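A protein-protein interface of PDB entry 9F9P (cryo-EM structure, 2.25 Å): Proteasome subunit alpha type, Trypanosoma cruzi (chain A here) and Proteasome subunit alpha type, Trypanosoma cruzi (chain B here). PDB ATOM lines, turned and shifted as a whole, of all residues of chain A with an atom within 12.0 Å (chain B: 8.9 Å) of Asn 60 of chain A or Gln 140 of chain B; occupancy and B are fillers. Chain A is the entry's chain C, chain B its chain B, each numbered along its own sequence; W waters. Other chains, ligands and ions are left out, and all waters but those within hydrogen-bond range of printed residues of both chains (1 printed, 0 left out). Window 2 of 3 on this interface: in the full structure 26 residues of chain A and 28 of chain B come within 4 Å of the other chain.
OG of Ser 58 of chain A lies within hydrogen-bond range of N of Asn 60 of chain A, at 2.9 Å. A ring nitrogen (NE2) of His 143 of chain B lies within hydrogen-bond range of the side-chain carboxylate (OD1) of Asp 138 of chain B (2.9 Å). O of Asn 142 of chain B is in hydrogen-bond range of NZ of Lys 37 of chain B. The backbone carbonyl oxygen (O) of Met 61 of chain A lies within hydrogen-bond range of the side-chain amino group (NZ) of Lys 64 of chain A, at 3.1 Å. The side-chain carboxylate of Asp 138 of chain B is in hydrogen-bond range of the backbone NH of Gln 140 of chain B (3.0 Å). O of Gly 136 of chain B sits at hydrogen-bond distance from N of His 143 of chain B (2.9 Å).
OH of Tyr 145 of chain B is in hydrogen-bond range of OE2 of Glu 59 of chain A (2.7 Å). The backbone carbonyl oxygen of Gln 140 of chain B sits at hydrogen-bond distance from the side-chain amide nitrogen of Asn 60 of chain A, at 3.0 Å. N of Asp 57 of chain A lies within hydrogen-bond range of O of Ala 155 of chain B, 3.1 Å away. The side-chain carboxylate of Asp 57 of chain A lies within salt-bridge range of the side-chain amino group of Lys 37 of chain B, 3.7 Å away.
Among the printed residues, merely in contact across the chains: Glu 59 of chain A with His 143 of chain B (3.4 Å), Met 61 of chain A with Ser 106 of chain B (3.9 Å) and Glu 59 of chain A with Ser 106 of chain B (3.9 Å).
Hydrophobic or aromatic side chains of chain A within 4 Å of the printed part of chain B: Met 61. Of the 14 printed residues of chain B, 6 touch a printed residue of chain A. Printed residues of chain B that touch a printed residue of chain A: Lys 37, Ser 106, Gln 140, His 143, Tyr 145 and Ala 155. Hydrophobic or aromatic side chains of chain B that line the printed part of chain A: His 143, Tyr 145 and Ala 155. Along chain B the printed residues that touch a printed residue of chain A span positions 37 to 155. Among the printed residues, Asp or Glu carboxylates within 4 Å of a Lys or Arg side-chain nitrogen of the other chain: Asp 57 of chain A with Lys 37 of chain B.
Of the printed residues of chain B, Asn 60 of chain A touches Gln 140 (3.0 Å). Of chain A, only Asn 60 (3.0 Å) comes within 4 Å of Gln 140 of chain B. No residue of chain A comes within 4 Å of Asp 138 of chain B. No residue of chain A comes within 4 Å of Ser 139 of chain B. No residue of chain A comes within 4 Å of Gly 141 of chain B. Of the printed residues of chain A, Tyr 145 of chain B touches Glu 59 (2.7 Å). Printed residues of chain B within 4 Å of Asp 57 of chain A: Lys 37 (3.0 Å) and Ala 155 (3.1 Å). Printed residues of chain B within 4 Å of Glu 59 of chain A: Ser 106, His 143 and Tyr 145. The nearest residue of chain B that does not touch Asn 60 of chain A is His 143 of chain B (4.8 Å). The nearest printed residue of chain B that does not touch Asp 57 of chain A is Asn 142 of chain B (5.2 Å).
Water W1 lies within hydrogen-bond range of O of Glu 59 of chain A (2.7 Å), OH of Tyr 145 of chain B (2.8 Å) and ND1 of His 143 of chain B (2.9 Å).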
ATOM      1  N   PHE A  56     -22.928 -15.085  -1.399  1.00  0.00           N
ATOM      2  CA  PHE A  56     -24.115 -14.506  -0.783  1.00  0.00           C
ATOM      3  C   PHE A  56     -23.732 -13.561   0.345  1.00  0.00           C
ATOM      4  O   PHE A  56     -22.706 -13.769   0.987  1.00  0.00           O
ATOM      5  CB  PHE A  56     -24.984 -15.583  -0.133  1.00  0.00           C
ATOM      6  CG  PHE A  56     -25.806 -16.458  -1.047  1.00  0.00           C
ATOM      7  CD1 PHE A  56     -25.964 -16.174  -2.399  1.00  0.00           C
ATOM      8  CD2 PHE A  56     -26.484 -17.559  -0.531  1.00  0.00           C
ATOM      9  CE1 PHE A  56     -26.744 -16.984  -3.217  1.00  0.00           C
ATOM     10  CE2 PHE A  56     -27.265 -18.369  -1.351  1.00  0.00           C
ATOM     11  CZ  PHE A  56     -27.384 -18.087  -2.696  1.00  0.00           C
ATOM     12  N   ASP A  57     -24.562 -12.542   0.575  1.00  0.00           N
ATOM     13  CA  ASP A  57     -24.327 -11.567   1.623  1.00  0.00           C
ATOM     14  C   ASP A  57     -25.578 -11.371   2.477  1.00  0.00           C
ATOM     15  O   ASP A  57     -26.672 -11.803   2.133  1.00  0.00           O
ATOM     16  CB  ASP A  57     -23.906 -10.212   1.055  1.00  0.00           C
ATOM     17  CG  ASP A  57     -23.096  -9.330   2.010  1.00  0.00           C
ATOM     18  OD1 ASP A  57     -22.588  -9.867   3.024  1.00  0.00           O
ATOM     19  OD2 ASP A  57     -22.956  -8.107   1.734  1.00  0.00           O
ATOM     20  N   SER A  58     -25.362 -10.747   3.633  1.00  0.00           N
ATOM     21  CA  SER A  58     -26.389 -10.281   4.544  1.00  0.00           C
ATOM     22  C   SER A  58     -26.881  -8.891   4.130  1.00  0.00           C
ATOM     23  O   SER A  58     -26.104  -8.071   3.645  1.00  0.00           O
ATOM     24  CB  SER A  58     -25.789 -10.249   5.942  1.00  0.00           C
ATOM     25  OG  SER A  58     -26.695  -9.734   6.913  1.00  0.00           O
ATOM     26  N   GLU A  59     -28.164  -8.607   4.371  1.00  0.00           N
ATOM     27  CA  GLU A  59     -28.670  -7.246   4.259  1.00  0.00           C
ATOM     28  C   GLU A  59     -28.140  -6.377   5.421  1.00  0.00           C
ATOM     29  O   GLU A  59     -28.161  -5.148   5.338  1.00  0.00           O
ATOM     30  CB  GLU A  59     -30.207  -7.249   4.178  1.00  0.00           C
ATOM     31  CG  GLU A  59     -30.841  -7.882   2.914  1.00  0.00           C
ATOM     32  CD  GLU A  59     -32.357  -7.604   2.708  1.00  0.00           C
ATOM     33  OE1 GLU A  59     -33.199  -8.515   2.985  1.00  0.00           O
ATOM     34  OE2 GLU A  59     -32.723  -6.475   2.267  1.00  0.00           O
ATOM     35  N   ASN A  60     -27.670  -6.999   6.505  1.00  0.00           N
ATOM     36  CA  ASN A  60     -27.202  -6.322   7.717  1.00  0.00           C
ATOM     37  C   ASN A  60     -28.264  -5.386   8.306  1.00  0.00           C
ATOM     38  O   ASN A  60     -27.971  -4.232   8.586  1.00  0.00           O
ATOM     39  CB  ASN A  60     -25.873  -5.599   7.513  1.00  0.00           C
ATOM     40  CG  ASN A  60     -25.217  -5.190   8.825  1.00  0.00           C
ATOM     41  OD1 ASN A  60     -25.129  -5.983   9.767  1.00  0.00           O
ATOM     42  ND2 ASN A  60     -24.768  -3.944   8.918  1.00  0.00           N
ATOM     43  N   MET A  61     -29.469  -5.909   8.570  1.00  0.00           N
ATOM     44  CA  MET A  61     -30.567  -5.149   9.162  1.00  0.00           C
ATOM     45  C   MET A  61     -30.339  -4.962  10.665  1.00  0.00           C
ATOM     46  O   MET A  61     -29.763  -5.820  11.321  1.00  0.00           O
ATOM     47  CB  MET A  61     -31.900  -5.890   8.962  1.00  0.00           C
ATOM     48  CG  MET A  61     -32.341  -6.048   7.489  1.00  0.00           C
ATOM     49  SD  MET A  61     -32.538  -4.469   6.586  1.00  0.00           S
ATOM     50  CE  MET A  61     -34.123  -4.770   5.797  1.00  0.00           C
ATOM     51  N   GLU A  62     -30.841  -3.848  11.220  1.00  0.00           N
ATOM     52  CA  GLU A  62     -30.554  -3.454  12.593  1.00  0.00           C
ATOM     53  C   GLU A  62     -31.243  -4.371  13.610  1.00  0.00           C
ATOM     54  O   GLU A  62     -30.621  -4.701  14.612  1.00  0.00           O
ATOM     55  CB  GLU A  62     -30.896  -1.972  12.760  1.00  0.00           C
ATOM     56  CG  GLU A  62     -30.640  -1.414  14.153  1.00  0.00           C
ATOM     57  CD  GLU A  62     -31.214  -0.021  14.440  1.00  0.00           C
ATOM     58  OE1 GLU A  62     -30.605   0.972  13.951  1.00  0.00           O
ATOM     59  OE2 GLU A  62     -32.288   0.074  15.153  1.00  0.00           O
ATOM     60  N   ASP A  63     -32.500  -4.796  13.362  1.00  0.00           N
ATOM     61  CA  ASP A  63     -33.240  -5.742  14.205  1.00  0.00           C
ATOM     62  C   ASP A  63     -33.393  -7.092  13.491  1.00  0.00           C
ATOM     63  O   ASP A  63     -33.928  -7.140  12.387  1.00  0.00           O
ATOM     64  CB  ASP A  63     -34.628  -5.164  14.537  1.00  0.00           C
ATOM     65  CG  ASP A  63     -35.598  -6.041  15.342  1.00  0.00           C
ATOM     66  OD1 ASP A  63     -35.281  -7.216  15.651  1.00  0.00           O
ATOM     67  OD2 ASP A  63     -36.676  -5.525  15.694  1.00  0.00           O
ATOM     68  N   LYS A  64     -33.003  -8.205  14.135  1.00  0.00           N
ATOM     69  CA  LYS A  64     -32.860  -9.480  13.434  1.00  0.00           C
ATOM     70  C   LYS A  64     -34.107 -10.371  13.501  1.00  0.00           C
ATOM     71  O   LYS A  64     -34.200 -11.331  12.738  1.00  0.00           O
ATOM     72  CB  LYS A  64     -31.664 -10.259  13.979  1.00  0.00           C
ATOM     73  CG  LYS A  64     -30.350  -9.489  14.029  1.00  0.00           C
ATOM     74  CD  LYS A  64     -29.653  -9.299  12.685  1.00  0.00           C
ATOM     75  CE  LYS A  64     -28.388  -8.471  12.827  1.00  0.00           C
ATOM     76  NZ  LYS A  64     -27.769  -8.157  11.514  1.00  0.00           N
ATOM     77  N   ASN A  65     -35.097 -10.043  14.334  1.00  0.00           N
ATOM     78  CA  ASN A  65     -36.261 -10.896  14.486  1.00  0.00           C
ATOM     79  C   ASN A  65     -37.491 -10.398  13.718  1.00  0.00           C
ATOM     80  O   ASN A  65     -38.614 -10.608  14.156  1.00  0.00           O
ATOM     81  CB  ASN A  65     -36.610 -11.026  15.970  1.00  0.00           C
ATOM     82  CG  ASN A  65     -35.488 -11.650  16.770  1.00  0.00           C
ATOM     83  OD1 ASN A  65     -35.375 -12.869  16.859  1.00  0.00           O
ATOM     84  ND2 ASN A  65     -34.661 -10.813  17.364  1.00  0.00           N
ATOM     85  N   ILE A  66     -37.329  -9.775  12.553  1.00  0.00           N
ATOM     86  CA  ILE A  66     -38.492  -9.306  11.813  1.00  0.00           C
ATOM     87  C   ILE A  66     -38.684 -10.155  10.559  1.00  0.00           C
ATOM     88  O   ILE A  66     -39.825 -10.376  10.149  1.00  0.00           O
ATOM     89  CB  ILE A  66     -38.360  -7.810  11.452  1.00  0.00           C
ATOM     90  CG1 ILE A  66     -38.146  -6.922  12.680  1.00  0.00           C
ATOM     91  CG2 ILE A  66     -39.519  -7.315  10.583  1.00  0.00           C
ATOM     92  CD1 ILE A  66     -39.378  -6.589  13.443  1.00  0.00           C
ATOM     93  N   SER A  67     -37.571 -10.514   9.895  1.00  0.00           N
ATOM     94  CA  SER A  67     -37.631 -11.293   8.671  1.00  0.00           C
ATOM     95  C   SER A  67     -36.336 -12.056   8.444  1.00  0.00           C
ATOM     96  O   SER A  67     -35.252 -11.501   8.584  1.00  0.00           O
ATOM     97  CB  SER A  67     -37.931 -10.426   7.479  1.00  0.00           C
ATOM     98  OG  SER A  67     -36.820  -9.612   7.144  1.00  0.00           O
ATOM     99  N   GLY A  68     -36.481 -13.338   8.099  1.00  0.00           N
ATOM    100  CA  GLY A  68     -35.420 -14.137   7.508  1.00  0.00           C
ATOM    101  C   GLY A  68     -35.689 -14.294   6.014  1.00  0.00           C
ATOM    102  O   GLY A  68     -36.371 -13.456   5.421  1.00  0.00           O
ATOM    103  N   GLU A  69     -35.198 -15.406   5.446  1.00  0.00           N
ATOM    104  CA  GLU A  69     -35.446 -15.771   4.057  1.00  0.00           C
ATOM    105  C   GLU A  69     -36.881 -16.268   3.903  1.00  0.00           C
ATOM    106  O   GLU A  69     -37.519 -16.014   2.883  1.00  0.00           O
ATOM    107  CB  GLU A  69     -34.479 -16.865   3.582  1.00  0.00           C
ATOM    108  CG  GLU A  69     -33.016 -16.425   3.478  1.00  0.00           C
ATOM    109  CD  GLU A  69     -32.285 -16.079   4.772  1.00  0.00           C
ATOM    110  OE1 GLU A  69     -32.801 -16.409   5.867  1.00  0.00           O
ATOM    111  OE2 GLU A  69     -31.198 -15.459   4.687  1.00  0.00           O
ATOM    112  N   ARG A 250     -30.988 -17.963  16.009  1.00  0.00           N
ATOM    113  CA  ARG A 250     -29.693 -17.738  15.381  1.00  0.00           C
ATOM    114  C   ARG A 250     -28.874 -19.022  15.485  1.00  0.00           C
ATOM    115  O   ARG A 250     -29.371 -20.021  15.995  1.00  0.00           O
ATOM    116  CB  ARG A 250     -28.999 -16.533  16.017  1.00  0.00           C
ATOM    117  CG  ARG A 250     -29.845 -15.269  16.022  1.00  0.00           C
ATOM    118  CD  ARG A 250     -29.024 -13.995  16.124  1.00  0.00           C
ATOM    119  NE  ARG A 250     -29.881 -12.835  16.356  1.00  0.00           N
ATOM    120  CZ  ARG A 250     -29.623 -11.840  17.202  1.00  0.00           C
ATOM    121  NH1 ARG A 250     -28.439 -11.745  17.783  1.00  0.00           N
ATOM    122  NH2 ARG A 250     -30.542 -10.916  17.435  1.00  0.00           N
ATOM    123  N   LYS B  37     -18.328  -5.913  -4.020  1.00  0.00           N
ATOM    124  CA  LYS B  37     -18.427  -5.186  -2.763  1.00  0.00           C
ATOM    125  C   LYS B  37     -17.106  -5.369  -2.039  1.00  0.00           C
ATOM    126  O   LYS B  37     -16.696  -6.491  -1.798  1.00  0.00           O
ATOM    127  CB  LYS B  37     -19.643  -5.705  -1.988  1.00  0.00           C
ATOM    128  CG  LYS B  37     -19.862  -5.141  -0.597  1.00  0.00           C
ATOM    129  CD  LYS B  37     -20.989  -5.877   0.088  1.00  0.00           C
ATOM    130  CE  LYS B  37     -20.814  -5.972   1.583  1.00  0.00           C
ATOM    131  NZ  LYS B  37     -21.362  -4.773   2.248  1.00  0.00           N
ATOM    132  N   PRO B 104     -32.740   4.212   2.637  1.00  0.00           N
ATOM    133  CA  PRO B 104     -31.878   3.038   2.667  1.00  0.00           C
ATOM    134  C   PRO B 104     -32.016   2.132   1.461  1.00  0.00           C
ATOM    135  O   PRO B 104     -33.101   1.956   0.950  1.00  0.00           O
ATOM    136  CB  PRO B 104     -32.343   2.249   3.890  1.00  0.00           C
ATOM    137  CG  PRO B 104     -33.050   3.254   4.724  1.00  0.00           C
ATOM    138  CD  PRO B 104     -33.717   4.171   3.720  1.00  0.00           C
ATOM    139  N   VAL B 105     -30.941   1.463   1.090  1.00  0.00           N
ATOM    140  CA  VAL B 105     -30.919   0.681  -0.134  1.00  0.00           C
ATOM    141  C   VAL B 105     -31.872  -0.512  -0.053  1.00  0.00           C
ATOM    142  O   VAL B 105     -32.524  -0.845  -1.015  1.00  0.00           O
ATOM    143  CB  VAL B 105     -29.493   0.207  -0.436  1.00  0.00           C
ATOM    144  CG1 VAL B 105     -29.413  -0.424  -1.789  1.00  0.00           C
ATOM    145  CG2 VAL B 105     -28.518   1.360  -0.380  1.00  0.00           C
ATOM    146  N   SER B 106     -31.967  -1.155   1.092  1.00  0.00           N
ATOM    147  CA  SER B 106     -32.980  -2.154   1.361  1.00  0.00           C
ATOM    148  C   SER B 106     -34.404  -1.681   1.039  1.00  0.00           C
ATOM    149  O   SER B 106     -35.214  -2.479   0.584  1.00  0.00           O
ATOM    150  CB  SER B 106     -32.887  -2.610   2.810  1.00  0.00           C
ATOM    151  OG  SER B 106     -33.327  -1.595   3.713  1.00  0.00           O
ATOM    152  N   GLY B 136     -25.130   0.832  -3.179  1.00  0.00           N
ATOM    153  CA  GLY B 136     -25.301   2.052  -2.406  1.00  0.00           C
ATOM    154  C   GLY B 136     -24.776   1.972  -0.992  1.00  0.00           C
ATOM    155  O   GLY B 136     -24.355   0.926  -0.578  1.00  0.00           O
ATOM    156  N   ALA B 137     -24.827   3.106  -0.298  1.00  0.00           N
ATOM    157  CA  ALA B 137     -24.358   3.245   1.076  1.00  0.00           C
ATOM    158  C   ALA B 137     -25.402   3.923   1.953  1.00  0.00           C
ATOM    159  O   ALA B 137     -26.003   4.911   1.547  1.00  0.00           O
ATOM    160  CB  ALA B 137     -23.104   4.067   1.089  1.00  0.00           C
ATOM    161  N   ASP B 138     -25.558   3.404   3.172  1.00  0.00           N
ATOM    162  CA  ASP B 138     -26.438   3.985   4.180  1.00  0.00           C
ATOM    163  C   ASP B 138     -25.894   3.674   5.582  1.00  0.00           C
ATOM    164  O   ASP B 138     -24.783   3.190   5.713  1.00  0.00           O
ATOM    165  CB  ASP B 138     -27.866   3.446   3.959  1.00  0.00           C
ATOM    166  CG  ASP B 138     -28.046   1.929   4.090  1.00  0.00           C
ATOM    167  OD1 ASP B 138     -27.190   1.285   4.723  1.00  0.00           O
ATOM    168  OD2 ASP B 138     -29.022   1.388   3.479  1.00  0.00           O
ATOM    169  N   SER B 139     -26.700   3.879   6.624  1.00  0.00           N
ATOM    170  CA  SER B 139     -26.305   3.660   8.014  1.00  0.00           C
ATOM    171  C   SER B 139     -25.857   2.236   8.312  1.00  0.00           C
ATOM    172  O   SER B 139     -25.002   2.036   9.176  1.00  0.00           O
ATOM    173  CB  SER B 139     -27.424   4.029   8.945  1.00  0.00           C
ATOM    174  OG  SER B 139     -27.767   5.400   8.780  1.00  0.00           O
ATOM    175  N   GLN B 140     -26.404   1.244   7.616  1.00  0.00           N
ATOM    176  CA  GLN B 140     -25.978  -0.134   7.821  1.00  0.00           C
ATOM    177  C   GLN B 140     -24.804  -0.535   6.922  1.00  0.00           C
ATOM    178  O   GLN B 140     -24.477  -1.714   6.861  1.00  0.00           O
ATOM    179  CB  GLN B 140     -27.134  -1.108   7.554  1.00  0.00           C
ATOM    180  CG  GLN B 140     -28.381  -0.858   8.400  1.00  0.00           C
ATOM    181  CD  GLN B 140     -28.078  -0.614   9.864  1.00  0.00           C
ATOM    182  OE1 GLN B 140     -28.379   0.458  10.387  1.00  0.00           O
ATOM    183  NE2 GLN B 140     -27.480  -1.597  10.527  1.00  0.00           N
ATOM    184  N   GLY B 141     -24.198   0.394   6.188  1.00  0.00           N
ATOM    185  CA  GLY B 141     -22.990   0.069   5.442  1.00  0.00           C
ATOM    186  C   GLY B 141     -23.154   0.137   3.921  1.00  0.00           C
ATOM    187  O   GLY B 141     -23.915   0.957   3.428  1.00  0.00           O
ATOM    188  N   ASN B 142     -22.381  -0.690   3.202  1.00  0.00           N
ATOM    189  CA  ASN B 142     -22.365  -0.720   1.752  1.00  0.00           C
ATOM    190  C   ASN B 142     -23.113  -1.944   1.255  1.00  0.00           C
ATOM    191  O   ASN B 142     -23.053  -2.959   1.898  1.00  0.00           O
ATOM    192  CB  ASN B 142     -20.938  -0.744   1.215  1.00  0.00           C
ATOM    193  CG  ASN B 142     -20.162   0.500   1.599  1.00  0.00           C
ATOM    194  OD1 ASN B 142     -20.515   1.631   1.269  1.00  0.00           O
ATOM    195  ND2 ASN B 142     -19.139   0.291   2.398  1.00  0.00           N
ATOM    196  N   HIS B 143     -23.895  -1.843   0.178  1.00  0.00           N
ATOM    197  CA  HIS B 143     -24.745  -2.963  -0.203  1.00  0.00           C
ATOM    198  C   HIS B 143     -24.708  -3.179  -1.699  1.00  0.00           C
ATOM    199  O   HIS B 143     -24.626  -2.226  -2.444  1.00  0.00           O
ATOM    200  CB  HIS B 143     -26.206  -2.734   0.191  1.00  0.00           C
ATOM    201  CG  HIS B 143     -26.422  -2.396   1.612  1.00  0.00           C
ATOM    202  ND1 HIS B 143     -26.253  -3.294   2.636  1.00  0.00           N
ATOM    203  CD2 HIS B 143     -26.683  -1.190   2.179  1.00  0.00           C
ATOM    204  CE1 HIS B 143     -26.447  -2.650   3.788  1.00  0.00           C
ATOM    205  NE2 HIS B 143     -26.707  -1.367   3.534  1.00  0.00           N
ATOM    206  N   TYR B 145     -27.138  -5.362  -4.534  1.00  0.00           N
ATOM    207  CA  TYR B 145     -28.260  -6.273  -4.703  1.00  0.00           C
ATOM    208  C   TYR B 145     -28.532  -6.579  -6.167  1.00  0.00           C
ATOM    209  O   TYR B 145     -28.192  -5.803  -7.009  1.00  0.00           O
ATOM    210  CB  TYR B 145     -29.559  -5.673  -4.186  1.00  0.00           C
ATOM    211  CG  TYR B 145     -29.742  -5.550  -2.702  1.00  0.00           C
ATOM    212  CD1 TYR B 145     -30.534  -6.438  -2.022  1.00  0.00           C
ATOM    213  CD2 TYR B 145     -29.312  -4.432  -2.021  1.00  0.00           C
ATOM    214  CE1 TYR B 145     -30.825  -6.297  -0.678  1.00  0.00           C
ATOM    215  CE2 TYR B 145     -29.559  -4.287  -0.661  1.00  0.00           C
ATOM    216  CZ  TYR B 145     -30.344  -5.215   0.006  1.00  0.00           C
ATOM    217  OH  TYR B 145     -30.611  -5.080   1.330  1.00  0.00           O
ATOM    218  N   ALA B 155     -29.092 -10.206  -1.989  1.00  0.00           N
ATOM    219  CA  ALA B 155     -27.892  -9.467  -1.621  1.00  0.00           C
ATOM    220  C   ALA B 155     -26.641 -10.281  -1.922  1.00  0.00           C
ATOM    221  O   ALA B 155     -26.575 -11.425  -1.573  1.00  0.00           O
ATOM    222  CB  ALA B 155     -27.960  -9.108  -0.160  1.00  0.00           C
HETATM  223  O   HOH W   1     -29.039  -3.700   3.226  1.00  0.00           O
